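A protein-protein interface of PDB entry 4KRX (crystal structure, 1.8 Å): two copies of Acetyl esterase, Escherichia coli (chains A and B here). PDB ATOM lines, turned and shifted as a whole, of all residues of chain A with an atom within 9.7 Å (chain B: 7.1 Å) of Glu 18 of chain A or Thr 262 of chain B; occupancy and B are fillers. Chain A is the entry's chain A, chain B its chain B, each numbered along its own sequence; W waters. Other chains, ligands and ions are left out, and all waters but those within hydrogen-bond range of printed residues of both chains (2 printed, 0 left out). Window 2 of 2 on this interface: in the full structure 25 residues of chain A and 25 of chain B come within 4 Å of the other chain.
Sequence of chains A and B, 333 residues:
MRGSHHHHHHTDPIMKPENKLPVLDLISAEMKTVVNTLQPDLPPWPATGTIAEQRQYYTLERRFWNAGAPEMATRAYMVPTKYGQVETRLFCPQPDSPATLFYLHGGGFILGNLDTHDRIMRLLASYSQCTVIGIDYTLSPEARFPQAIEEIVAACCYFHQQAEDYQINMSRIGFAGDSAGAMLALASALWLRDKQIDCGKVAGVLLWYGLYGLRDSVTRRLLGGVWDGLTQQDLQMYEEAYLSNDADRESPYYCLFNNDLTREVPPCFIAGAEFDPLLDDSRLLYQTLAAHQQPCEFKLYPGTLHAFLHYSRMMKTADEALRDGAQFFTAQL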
ATOM      1  N   GLU A  18      -8.044   1.754  -0.367  1.00  0.00           N
ATOM      2  CA  GLU A  18      -9.524   1.570  -0.409  1.00  0.00           C
ATOM      3  C   GLU A  18     -10.065   2.324   0.821  1.00  0.00           C
ATOM      4  O   GLU A  18     -10.389   3.533   0.696  1.00  0.00           O
ATOM      5  CB  GLU A  18      -9.930   0.067  -0.517  1.00  0.00           C
ATOM      6  CG  GLU A  18      -9.194  -0.988   0.330  1.00  0.00           C
ATOM      7  CD  GLU A  18      -7.667  -1.040   0.158  1.00  0.00           C
ATOM      8  OE1 GLU A  18      -6.966  -0.066   0.525  1.00  0.00           O
ATOM      9  OE2 GLU A  18      -7.141  -2.075  -0.311  1.00  0.00           O
ATOM     10  N   ASN A  19     -10.000   1.719   2.031  1.00  0.00           N
ATOM     11  CA  ASN A  19     -10.445   2.475   3.180  1.00  0.00           C
ATOM     12  C   ASN A  19      -9.389   3.314   3.898  1.00  0.00           C
ATOM     13  O   ASN A  19      -9.616   3.770   5.063  1.00  0.00           O
ATOM     14  CB  ASN A  19     -11.076   1.568   4.196  1.00  0.00           C
ATOM     15  CG  ASN A  19     -12.216   0.767   3.643  1.00  0.00           C
ATOM     16  OD1 ASN A  19     -12.989   1.182   2.763  1.00  0.00           O
ATOM     17  ND2 ASN A  19     -12.355  -0.352   4.168  1.00  0.00           N
ATOM     18  N   LYS A  20      -8.242   3.490   3.286  1.00  0.00           N
ATOM     19  CA  LYS A  20      -7.151   4.193   3.947  1.00  0.00           C
ATOM     20  C   LYS A  20      -7.362   5.671   4.011  1.00  0.00           C
ATOM     21  O   LYS A  20      -8.148   6.264   3.179  1.00  0.00           O
ATOM     22  CB  LYS A  20      -5.857   3.875   3.238  1.00  0.00           C
ATOM     23  CG  LYS A  20      -5.555   2.397   3.213  1.00  0.00           C
ATOM     24  CD  LYS A  20      -4.435   2.060   4.109  1.00  0.00           C
ATOM     25  CE  LYS A  20      -3.992   0.606   4.059  1.00  0.00           C
ATOM     26  NZ  LYS A  20      -3.798   0.178   5.484  1.00  0.00           N
ATOM     27  N   LEU A  21      -6.709   6.321   4.943  1.00  0.00           N
ATOM     28  CA  LEU A  21      -6.661   7.781   4.978  1.00  0.00           C
ATOM     29  C   LEU A  21      -5.896   8.354   3.785  1.00  0.00           C
ATOM     30  O   LEU A  21      -4.987   7.688   3.243  1.00  0.00           O
ATOM     31  CB  LEU A  21      -6.016   8.316   6.251  1.00  0.00           C
ATOM     32  CG  LEU A  21      -6.746   7.905   7.520  1.00  0.00           C
ATOM     33  CD1 LEU A  21      -6.036   8.411   8.763  1.00  0.00           C
ATOM     34  CD2 LEU A  21      -8.161   8.408   7.438  1.00  0.00           C
ATOM     35  N   PRO A  22      -6.265   9.611   3.367  1.00  0.00           N
ATOM     36  CA  PRO A  22      -5.577  10.253   2.232  1.00  0.00           C
ATOM     37  C   PRO A  22      -4.246  10.858   2.759  1.00  0.00           C
ATOM     38  O   PRO A  22      -4.095  12.077   2.910  1.00  0.00           O
ATOM     39  CB  PRO A  22      -6.614  11.320   1.751  1.00  0.00           C
ATOM     40  CG  PRO A  22      -7.280  11.723   3.031  1.00  0.00           C
ATOM     41  CD  PRO A  22      -7.352  10.451   3.881  1.00  0.00           C
ATOM     42  N   ARG A 220      -2.470   0.263  11.335  1.00  0.00           N
ATOM     43  CA  ARG A 220      -2.133  -0.576  10.161  1.00  0.00           C
ATOM     44  C   ARG A 220      -3.265  -0.579   9.181  1.00  0.00           C
ATOM     45  O   ARG A 220      -3.019  -0.615   7.932  1.00  0.00           O
ATOM     46  CB  ARG A 220      -1.787  -1.991  10.569  1.00  0.00           C
ATOM     47  CG  ARG A 220      -0.379  -1.985  11.162  1.00  0.00           C
ATOM     48  CD  ARG A 220      -0.124  -3.327  11.846  1.00  0.00           C
ATOM     49  NE  ARG A 220       1.095  -3.276  12.642  1.00  0.00           N
ATOM     50  CZ  ARG A 220       2.120  -4.089  12.467  1.00  0.00           C
ATOM     51  NH1 ARG A 220       2.071  -4.994  11.439  1.00  0.00           N
ATOM     52  NH2 ARG A 220       3.156  -4.010  13.303  1.00  0.00           N
ATOM     53  N   ARG A 221      -4.495  -0.533   9.693  1.00  0.00           N
ATOM     54  CA  ARG A 221      -5.657  -0.536   8.764  1.00  0.00           C
ATOM     55  C   ARG A 221      -5.828   0.810   8.078  1.00  0.00           C
ATOM     56  O   ARG A 221      -6.172   0.883   6.909  1.00  0.00           O
ATOM     57  CB  ARG A 221      -6.929  -0.922   9.530  1.00  0.00           C
ATOM     58  CG  ARG A 221      -6.930  -2.388   9.955  1.00  0.00           C
ATOM     59  CD  ARG A 221      -7.260  -3.297   8.749  1.00  0.00           C
ATOM     60  NE  ARG A 221      -7.192  -4.674   9.139  1.00  0.00           N
ATOM     61  CZ  ARG A 221      -7.685  -5.738   8.507  1.00  0.00           C
ATOM     62  NH1 ARG A 221      -8.259  -5.657   7.319  1.00  0.00           N
ATOM     63  NH2 ARG A 221      -7.475  -6.925   9.086  1.00  0.00           N
ATOM     64  N   LEU A 222      -5.686   1.899   8.825  1.00  0.00           N
ATOM     65  CA  LEU A 222      -5.850   3.246   8.292  1.00  0.00           C
ATOM     66  C   LEU A 222      -4.706   3.789   7.389  1.00  0.00           C
ATOM     67  O   LEU A 222      -4.955   4.703   6.526  1.00  0.00           O
ATOM     68  CB  LEU A 222      -6.016   4.174   9.474  1.00  0.00           C
ATOM     69  CG  LEU A 222      -7.384   4.103  10.167  1.00  0.00           C
ATOM     70  CD1 LEU A 222      -7.412   4.953  11.424  1.00  0.00           C
ATOM     71  CD2 LEU A 222      -8.487   4.563   9.210  1.00  0.00           C
ATOM     72  N   LEU A 223      -3.470   3.253   7.546  1.00  0.00           N
ATOM     73  CA  LEU A 223      -2.282   3.887   6.993  1.00  0.00           C
ATOM     74  C   LEU A 223      -1.436   2.942   6.219  1.00  0.00           C
ATOM     75  O   LEU A 223      -1.694   1.735   6.248  1.00  0.00           O
ATOM     76  CB  LEU A 223      -1.468   4.595   8.102  1.00  0.00           C
ATOM     77  CG  LEU A 223      -2.261   5.634   8.896  1.00  0.00           C
ATOM     78  CD1 LEU A 223      -1.569   5.960  10.200  1.00  0.00           C
ATOM     79  CD2 LEU A 223      -2.447   6.932   8.225  1.00  0.00           C
ATOM     80  N   GLY A 224      -0.404   3.439   5.547  1.00  0.00           N
ATOM     81  CA  GLY A 224       0.456   2.594   4.712  1.00  0.00           C
ATOM     82  C   GLY A 224       0.098   2.639   3.231  1.00  0.00           C
ATOM     83  O   GLY A 224      -1.062   2.596   2.865  1.00  0.00           O
ATOM     84  N   GLY A 225       1.098   2.738   2.382  1.00  0.00           N
ATOM     85  CA  GLY A 225       0.841   2.832   0.923  1.00  0.00           C
ATOM     86  C   GLY A 225       2.166   2.862   0.183  1.00  0.00           C
ATOM     87  O   GLY A 225       3.229   2.606   0.739  1.00  0.00           O
ATOM     88  N   TRP A 227       3.815   5.349  -0.754  1.00  0.00           N
ATOM     89  CA  TRP A 227       4.650   6.441  -0.262  1.00  0.00           C
ATOM     90  C   TRP A 227       5.554   6.036   0.887  1.00  0.00           C
ATOM     91  O   TRP A 227       6.578   6.655   1.125  1.00  0.00           O
ATOM     92  CB  TRP A 227       3.788   7.586   0.233  1.00  0.00           C
ATOM     93  CG  TRP A 227       2.660   7.175   1.175  1.00  0.00           C
ATOM     94  CD1 TRP A 227       2.729   7.026   2.564  1.00  0.00           C
ATOM     95  CD2 TRP A 227       1.354   6.803   0.799  1.00  0.00           C
ATOM     96  NE1 TRP A 227       1.508   6.651   3.043  1.00  0.00           N
ATOM     97  CE2 TRP A 227       0.648   6.486   1.980  1.00  0.00           C
ATOM     98  CE3 TRP A 227       0.674   6.740  -0.439  1.00  0.00           C
ATOM     99  CZ2 TRP A 227      -0.674   6.048   1.962  1.00  0.00           C
ATOM    100  CZ3 TRP A 227      -0.656   6.321  -0.448  1.00  0.00           C
ATOM    101  CH2 TRP A 227      -1.324   6.017   0.740  1.00  0.00           C
ATOM    102  N   THR A 231       2.321  -1.181   3.279  1.00  0.00           N
ATOM    103  CA  THR A 231       1.005  -1.817   3.144  1.00  0.00           C
ATOM    104  C   THR A 231       1.073  -3.135   3.866  1.00  0.00           C
ATOM    105  O   THR A 231       2.147  -3.620   4.085  1.00  0.00           O
ATOM    106  CB  THR A 231       0.692  -2.192   1.709  1.00  0.00           C
ATOM    107  OG1 THR A 231       1.710  -3.075   1.229  1.00  0.00           O
ATOM    108  CG2 THR A 231       0.688  -0.947   0.848  1.00  0.00           C
ATOM    109  N   GLN A 232      -0.073  -3.716   4.173  1.00  0.00           N
ATOM    110  CA  GLN A 232      -0.132  -5.060   4.774  1.00  0.00           C
ATOM    111  C   GLN A 232       0.753  -6.022   4.027  1.00  0.00           C
ATOM    112  O   GLN A 232       1.426  -6.844   4.639  1.00  0.00           O
ATOM    113  CB  GLN A 232      -1.577  -5.614   4.823  1.00  0.00           C
ATOM    114  CG  GLN A 232      -1.728  -6.914   5.657  1.00  0.00           C
ATOM    115  CD  GLN A 232      -3.209  -7.292   5.945  1.00  0.00           C
ATOM    116  OE1 GLN A 232      -4.045  -7.312   5.028  1.00  0.00           O
ATOM    117  NE2 GLN A 232      -3.531  -7.581   7.224  1.00  0.00           N
ATOM    118  N   GLN A 233       0.650  -6.013   2.702  1.00  0.00           N
ATOM    119  CA  GLN A 233       1.427  -6.921   1.851  1.00  0.00           C
ATOM    120  C   GLN A 233       2.936  -6.704   1.958  1.00  0.00           C
ATOM    121  O   GLN A 233       3.729  -7.656   1.921  1.00  0.00           O
ATOM    122  CB  GLN A 233       0.987  -6.771   0.380  1.00  0.00           C
ATOM    123  CG  GLN A 233       1.622  -7.770  -0.566  1.00  0.00           C
ATOM    124  CD  GLN A 233       1.579  -7.353  -2.047  1.00  0.00           C
ATOM    125  OE1 GLN A 233       1.741  -6.174  -2.396  1.00  0.00           O
ATOM    126  NE2 GLN A 233       1.391  -8.338  -2.927  1.00  0.00           N
ATOM    127  N   ARG B 193     -26.598  -3.676   0.790  1.00  0.00           N
ATOM    128  CA  ARG B 193     -26.028  -2.624  -0.099  1.00  0.00           C
ATOM    129  C   ARG B 193     -25.323  -3.254  -1.315  1.00  0.00           C
ATOM    130  O   ARG B 193     -25.595  -2.902  -2.490  1.00  0.00           O
ATOM    131  CB  ARG B 193     -25.031  -1.734   0.666  1.00  0.00           C
ATOM    132  CG  ARG B 193     -24.316  -0.706  -0.241  1.00  0.00           C
ATOM    133  CD  ARG B 193     -23.102  -0.144   0.506  1.00  0.00           C
ATOM    134  NE  ARG B 193     -22.039  -1.139   0.654  1.00  0.00           N
ATOM    135  CZ  ARG B 193     -20.842  -0.870   1.148  1.00  0.00           C
ATOM    136  NH1 ARG B 193     -20.579   0.348   1.628  1.00  0.00           N
ATOM    137  NH2 ARG B 193     -19.936  -1.842   1.234  1.00  0.00           N
ATOM    138  N   PHE B 257     -13.651  -4.455   7.542  1.00  0.00           N
ATOM    139  CA  PHE B 257     -12.631  -3.538   7.103  1.00  0.00           C
ATOM    140  C   PHE B 257     -12.074  -3.899   5.734  1.00  0.00           C
ATOM    141  O   PHE B 257     -11.436  -3.046   5.126  1.00  0.00           O
ATOM    142  CB  PHE B 257     -11.496  -3.558   8.129  1.00  0.00           C
ATOM    143  CG  PHE B 257     -11.961  -3.215   9.548  1.00  0.00           C
ATOM    144  CD1 PHE B 257     -12.585  -2.022   9.756  1.00  0.00           C
ATOM    145  CD2 PHE B 257     -11.812  -4.071  10.617  1.00  0.00           C
ATOM    146  CE1 PHE B 257     -13.083  -1.643  10.937  1.00  0.00           C
ATOM    147  CE2 PHE B 257     -12.312  -3.715  11.848  1.00  0.00           C
ATOM    148  CZ  PHE B 257     -12.897  -2.488  12.048  1.00  0.00           C
ATOM    149  N   ASN B 258     -12.346  -5.109   5.244  1.00  0.00           N
ATOM    150  CA  ASN B 258     -12.041  -5.459   3.822  1.00  0.00           C
ATOM    151  C   ASN B 258     -13.165  -5.167   2.872  1.00  0.00           C
ATOM    152  O   ASN B 258     -13.010  -5.408   1.669  1.00  0.00           O
ATOM    153  CB  ASN B 258     -11.703  -6.931   3.671  1.00  0.00           C
ATOM    154  CG  ASN B 258     -10.375  -7.287   4.334  1.00  0.00           C
ATOM    155  OD1 ASN B 258      -9.573  -6.412   4.631  1.00  0.00           O
ATOM    156  ND2 ASN B 258     -10.108  -8.537   4.491  1.00  0.00           N
ATOM    157  N   ASN B 259     -14.318  -4.756   3.387  1.00  0.00           N
ATOM    158  CA  ASN B 259     -15.400  -4.306   2.549  1.00  0.00           C
ATOM    159  C   ASN B 259     -15.139  -2.849   2.267  1.00  0.00           C
ATOM    160  O   ASN B 259     -14.245  -2.269   2.835  1.00  0.00           O
ATOM    161  CB  ASN B 259     -16.747  -4.554   3.228  1.00  0.00           C
ATOM    162  CG  ASN B 259     -17.908  -4.701   2.217  1.00  0.00           C
ATOM    163  OD1 ASN B 259     -17.934  -4.009   1.213  1.00  0.00           O
ATOM    164  ND2 ASN B 259     -18.834  -5.606   2.485  1.00  0.00           N
ATOM    165  N   ASP B 260     -15.857  -2.238   1.290  1.00  0.00           N
ATOM    166  CA  ASP B 260     -15.755  -0.815   1.079  1.00  0.00           C
ATOM    167  C   ASP B 260     -16.579  -0.034   2.114  1.00  0.00           C
ATOM    168  O   ASP B 260     -17.808  -0.197   2.218  1.00  0.00           O
ATOM    169  CB  ASP B 260     -16.299  -0.544  -0.351  1.00  0.00           C
ATOM    170  CG  ASP B 260     -16.294   0.889  -0.750  1.00  0.00           C
ATOM    171  OD1 ASP B 260     -15.804   1.793  -0.072  1.00  0.00           O
ATOM    172  OD2 ASP B 260     -16.789   1.115  -1.864  1.00  0.00           O
ATOM    173  N   LEU B 261     -15.900   0.796   2.901  1.00  0.00           N
ATOM    174  CA  LEU B 261     -16.489   1.585   3.979  1.00  0.00           C
ATOM    175  C   LEU B 261     -16.429   3.059   3.629  1.00  0.00           C
ATOM    176  O   LEU B 261     -16.504   3.908   4.485  1.00  0.00           O
ATOM    177  CB  LEU B 261     -15.737   1.344   5.315  1.00  0.00           C
ATOM    178  CG  LEU B 261     -15.857  -0.098   5.807  1.00  0.00           C
ATOM    179  CD1 LEU B 261     -15.119  -0.310   7.111  1.00  0.00           C
ATOM    180  CD2 LEU B 261     -17.298  -0.521   6.000  1.00  0.00           C
ATOM    181  N   THR B 262     -16.324   3.372   2.333  1.00  0.00           N
ATOM    182  CA  THR B 262     -16.069   4.751   1.944  1.00  0.00           C
ATOM    183  C   THR B 262     -17.309   5.355   1.290  1.00  0.00           C
ATOM    184  O   THR B 262     -17.280   6.556   0.990  1.00  0.00           O
ATOM    185  CB  THR B 262     -14.896   4.894   0.922  1.00  0.00           C
ATOM    186  OG1 THR B 262     -15.280   4.326  -0.347  1.00  0.00           O
ATOM    187  CG2 THR B 262     -13.665   4.190   1.406  1.00  0.00           C
ATOM    188  N   ARG B 263     -18.345   4.552   1.101  1.00  0.00           N
ATOM    189  CA  ARG B 263     -19.555   5.028   0.477  1.00  0.00           C
ATOM    190  C   ARG B 263     -20.756   4.233   0.851  1.00  0.00           C
ATOM    191  O   ARG B 263     -20.710   3.014   1.023  1.00  0.00           O
ATOM    192  CB  ARG B 263     -19.304   5.038  -1.046  1.00  0.00           C
ATOM    193  CG  ARG B 263     -19.074   3.706  -1.693  1.00  0.00           C
ATOM    194  CD  ARG B 263     -18.696   3.904  -3.185  1.00  0.00           C
ATOM    195  NE  ARG B 263     -19.851   3.845  -4.080  1.00  0.00           N
ATOM    196  CZ  ARG B 263     -20.102   4.663  -5.134  1.00  0.00           C
ATOM    197  NH1 ARG B 263     -19.318   5.732  -5.448  1.00  0.00           N
ATOM    198  NH2 ARG B 263     -21.195   4.427  -5.860  1.00  0.00           N
ATOM    199  N   GLU B 264     -21.892   4.934   0.883  1.00  0.00           N
ATOM    200  CA  GLU B 264     -23.207   4.355   1.103  1.00  0.00           C
ATOM    201  C   GLU B 264     -23.303   3.442   2.337  1.00  0.00           C
ATOM    202  O   GLU B 264     -23.941   2.424   2.339  1.00  0.00           O
ATOM    203  CB  GLU B 264     -23.687   3.585  -0.128  1.00  0.00           C
ATOM    204  CG  GLU B 264     -23.966   4.530  -1.278  1.00  0.00           C
ATOM    205  CD  GLU B 264     -24.302   3.753  -2.563  1.00  0.00           C
ATOM    206  OE1 GLU B 264     -23.359   3.257  -3.221  1.00  0.00           O
ATOM    207  OE2 GLU B 264     -25.488   3.695  -2.908  1.00  0.00           O
ATOM    208  N   VAL B 265     -22.624   3.833   3.378  1.00  0.00           N
ATOM    209  CA  VAL B 265     -22.791   3.065   4.607  1.00  0.00           C
ATOM    210  C   VAL B 265     -23.926   3.793   5.394  1.00  0.00           C
ATOM    211  O   VAL B 265     -23.866   5.015   5.625  1.00  0.00           O
ATOM    212  CB  VAL B 265     -21.478   3.054   5.441  1.00  0.00           C
ATOM    213  CG1 VAL B 265     -21.693   2.179   6.660  1.00  0.00           C
ATOM    214  CG2 VAL B 265     -20.311   2.554   4.605  1.00  0.00           C
ATOM    215  N   THR B 288     -12.659   5.191  10.423  1.00  0.00           N
ATOM    216  CA  THR B 288     -12.763   4.873   8.954  1.00  0.00           C
ATOM    217  C   THR B 288     -13.956   5.581   8.388  1.00  0.00           C
ATOM    218  O   THR B 288     -13.837   6.285   7.260  1.00  0.00           O
ATOM    219  CB  THR B 288     -12.895   3.367   8.694  1.00  0.00           C
ATOM    220  OG1 THR B 288     -11.749   2.682   9.191  1.00  0.00           O
ATOM    221  CG2 THR B 288     -12.874   3.098   7.208  1.00  0.00           C
ATOM    222  N   LEU B 289     -15.093   5.413   9.052  1.00  0.00           N
ATOM    223  CA  LEU B 289     -16.333   6.041   8.500  1.00  0.00           C
ATOM    224  C   LEU B 289     -16.218   7.505   8.532  1.00  0.00           C
ATOM    225  O   LEU B 289     -16.555   8.170   7.478  1.00  0.00           O
ATOM    226  CB  LEU B 289     -17.574   5.578   9.249  1.00  0.00           C
ATOM    227  CG  LEU B 289     -17.902   4.085   9.203  1.00  0.00           C
ATOM    228  CD1 LEU B 289     -19.064   3.731  10.111  1.00  0.00           C
ATOM    229  CD2 LEU B 289     -18.200   3.615   7.777  1.00  0.00           C
ATOM    230  N   HIS B 292     -14.216   9.117   5.697  1.00  0.00           N
ATOM    231  CA  HIS B 292     -14.790   9.084   4.373  1.00  0.00           C
ATOM    232  C   HIS B 292     -16.137   9.786   4.346  1.00  0.00           C
ATOM    233  O   HIS B 292     -16.974   9.424   3.537  1.00  0.00           O
ATOM    234  CB  HIS B 292     -14.837   7.612   3.914  1.00  0.00           C
ATOM    235  CG  HIS B 292     -13.473   7.097   3.624  1.00  0.00           C
ATOM    236  ND1 HIS B 292     -12.737   6.334   4.533  1.00  0.00           N
ATOM    237  CD2 HIS B 292     -12.623   7.396   2.621  1.00  0.00           C
ATOM    238  CE1 HIS B 292     -11.531   6.108   4.042  1.00  0.00           C
ATOM    239  NE2 HIS B 292     -11.437   6.770   2.892  1.00  0.00           N
ATOM    240  N   GLN B 293     -16.368  10.651   5.318  1.00  0.00           N
ATOM    241  CA  GLN B 293     -17.619  11.397   5.443  1.00  0.00           C
ATOM    242  C   GLN B 293     -18.852  10.503   5.534  1.00  0.00           C
ATOM    243  O   GLN B 293     -19.926  10.880   5.036  1.00  0.00           O
ATOM    244  CB  GLN B 293     -17.696  12.427   4.244  1.00  0.00           C
ATOM    245  CG  GLN B 293     -16.558  13.436   4.302  1.00  0.00           C
ATOM    246  CD  GLN B 293     -15.275  12.905   3.644  1.00  0.00           C
ATOM    247  OE1 GLN B 293     -15.318  12.264   2.574  1.00  0.00           O
ATOM    248  NE2 GLN B 293     -14.126  13.134   4.303  1.00  0.00           N
ATOM    249  N   GLN B 294     -18.734   9.290   6.114  1.00  0.00           N
ATOM    250  CA  GLN B 294     -19.877   8.477   6.284  1.00  0.00           C
ATOM    251  C   GLN B 294     -20.526   8.778   7.671  1.00  0.00           C
ATOM    252  O   GLN B 294     -19.821   9.067   8.623  1.00  0.00           O
ATOM    253  CB  GLN B 294     -19.584   6.989   6.098  1.00  0.00           C
ATOM    254  CG  GLN B 294     -18.956   6.524   4.792  1.00  0.00           C
ATOM    255  CD  GLN B 294     -19.941   6.871   3.663  1.00  0.00           C
ATOM    256  OE1 GLN B 294     -21.016   6.321   3.583  1.00  0.00           O
ATOM    257  NE2 GLN B 294     -19.597   7.832   2.897  1.00  0.00           N
HETATM  258  O   HOH W   1      -8.516  -3.256   5.548  1.00  0.00           O
HETATM  259  O   HOH W   2      -9.610   1.761   7.480  1.00  0.00           O
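The side-chain amide nitrogen of Asn 19 of chain A sits at hydrogen-bond distance from the backbone carbonyl oxygen of Phe 257 of chain B. ND2 of Asn 19 of chain A sits at hydrogen-bond distance from O of Asn 259 of chain B (3.0 Å). OD1 of Asn 19 of chain A sits at hydrogen-bond distance from N of Leu 261 of chain B, at 2.9 Å. O of Lys 20 of chain A is in hydrogen-bond range of NE2 of His 292 of chain B. The side-chain amide oxygen (OD1) of Asn 258 of chain B lies within hydrogen-bond range of the guanidinium group (NH1) of Arg 221 of chain A (3.1 Å).
Among the printed residues, merely in contact across the chains: Glu 18 of chain A with Thr 262 of chain B (3.4 Å), Asn 19 of chain A with Asp 260 of chain B (3.8 Å), Asn 19 of chain A with Thr 262 of chain B (3.4 Å), Asn 19 of chain A with Thr 288 of chain B (3.8 Å), Asn 19 of chain A with His 292 of chain B (3.2 Å), Arg 221 of chain A with Phe 257 of chain B (3.9 Å) and Leu 222 of chain A with Thr 288 of chain B (3.8 Å).
Of chain B, only Thr 262 (3.4 Å) comes within 4 Å of Glu 18 of chain A. Of chain A, only Glu 18 and Asn 19 come within 4 Å of Thr 262 of chain B. Of the printed residues of chain A, Asp 260 of chain B touches Asn 19 (3.8 Å). Of the printed residues of chain A, Thr 288 of chain B touches Asn 19 and Leu 222. Of the printed residues of chain A, Phe 257 of chain B touches Asn 19 and Arg 221. Of the printed residues of chain A, Leu 261 of chain B touches Asn 19. Arg 220 of chain A touches none of the printed residues of chain B. The nearest printed residue of chain B that does not touch Leu 222 of chain A is His 292 of chain B (6.2 Å).
No position is printed for both chains. Of the 12 pairs that touch across the chains among the printed residues, none has its exchanged pair printed and touching as well.
The backbone carbonyl oxygen (O) of Arg 220 of chain A lies within hydrogen-bond range of the side-chain amino group (NZ) of Lys 20 of chain A. O of Arg 221 of chain A sits at hydrogen-bond distance from NZ of Lys 20 of chain A. The guanidinium group (NH2) of Arg 193 of chain B sits at hydrogen-bond distance from the side-chain amide oxygen (OD1) of Asn 259 of chain B (3.0 Å). The backbone carbonyl oxygen (O) of Asp 260 of chain B sits at hydrogen-bond distance from the guanidinium group (NH2) of Arg 193 of chain B. The side-chain carboxylate (OD1) of Asp 260 of chain B sits at hydrogen-bond distance from the side-chain hydroxyl (OG1) of Thr 262 of chain B, 2.6 Å away. The side-chain amide nitrogen (NE2) of Gln 294 of chain B is in hydrogen-bond range of the backbone carbonyl oxygen (O) of His 292 of chain B, 3.1 Å away.
Of the 15 printed residues of chain A, 5 touch a printed residue of chain B. Printed residues of chain A that touch a printed residue of chain B: Glu 18, Asn 19, Lys 20, Arg 221 and Leu 222. Hydrophobic or aromatic side chains of chain A within 4 Å of the printed part of chain B: Leu 222. Among the printed residues, 12 pairs touch across the chains. Among the printed residues, no Asp or Glu carboxylate lies within 4 Å of a Lys or Arg side-chain nitrogen of the other chain.
Water W2 lies within hydrogen-bond range of the side-chain hydroxyl (OG1) of Thr 288 of chain B and the backbone carbonyl oxygen (O) of Asn 19 of chain A. Water W1 lies within hydrogen-bond range of the backbone carbonyl oxygen (O) of Phe 257 of chain B (3.0 Å), the guanidinium group (NH1) of Arg 221 of chain A (3.0 Å) and the side-chain amide oxygen (OD1) of Asn 258 of chain B (3.5 Å).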
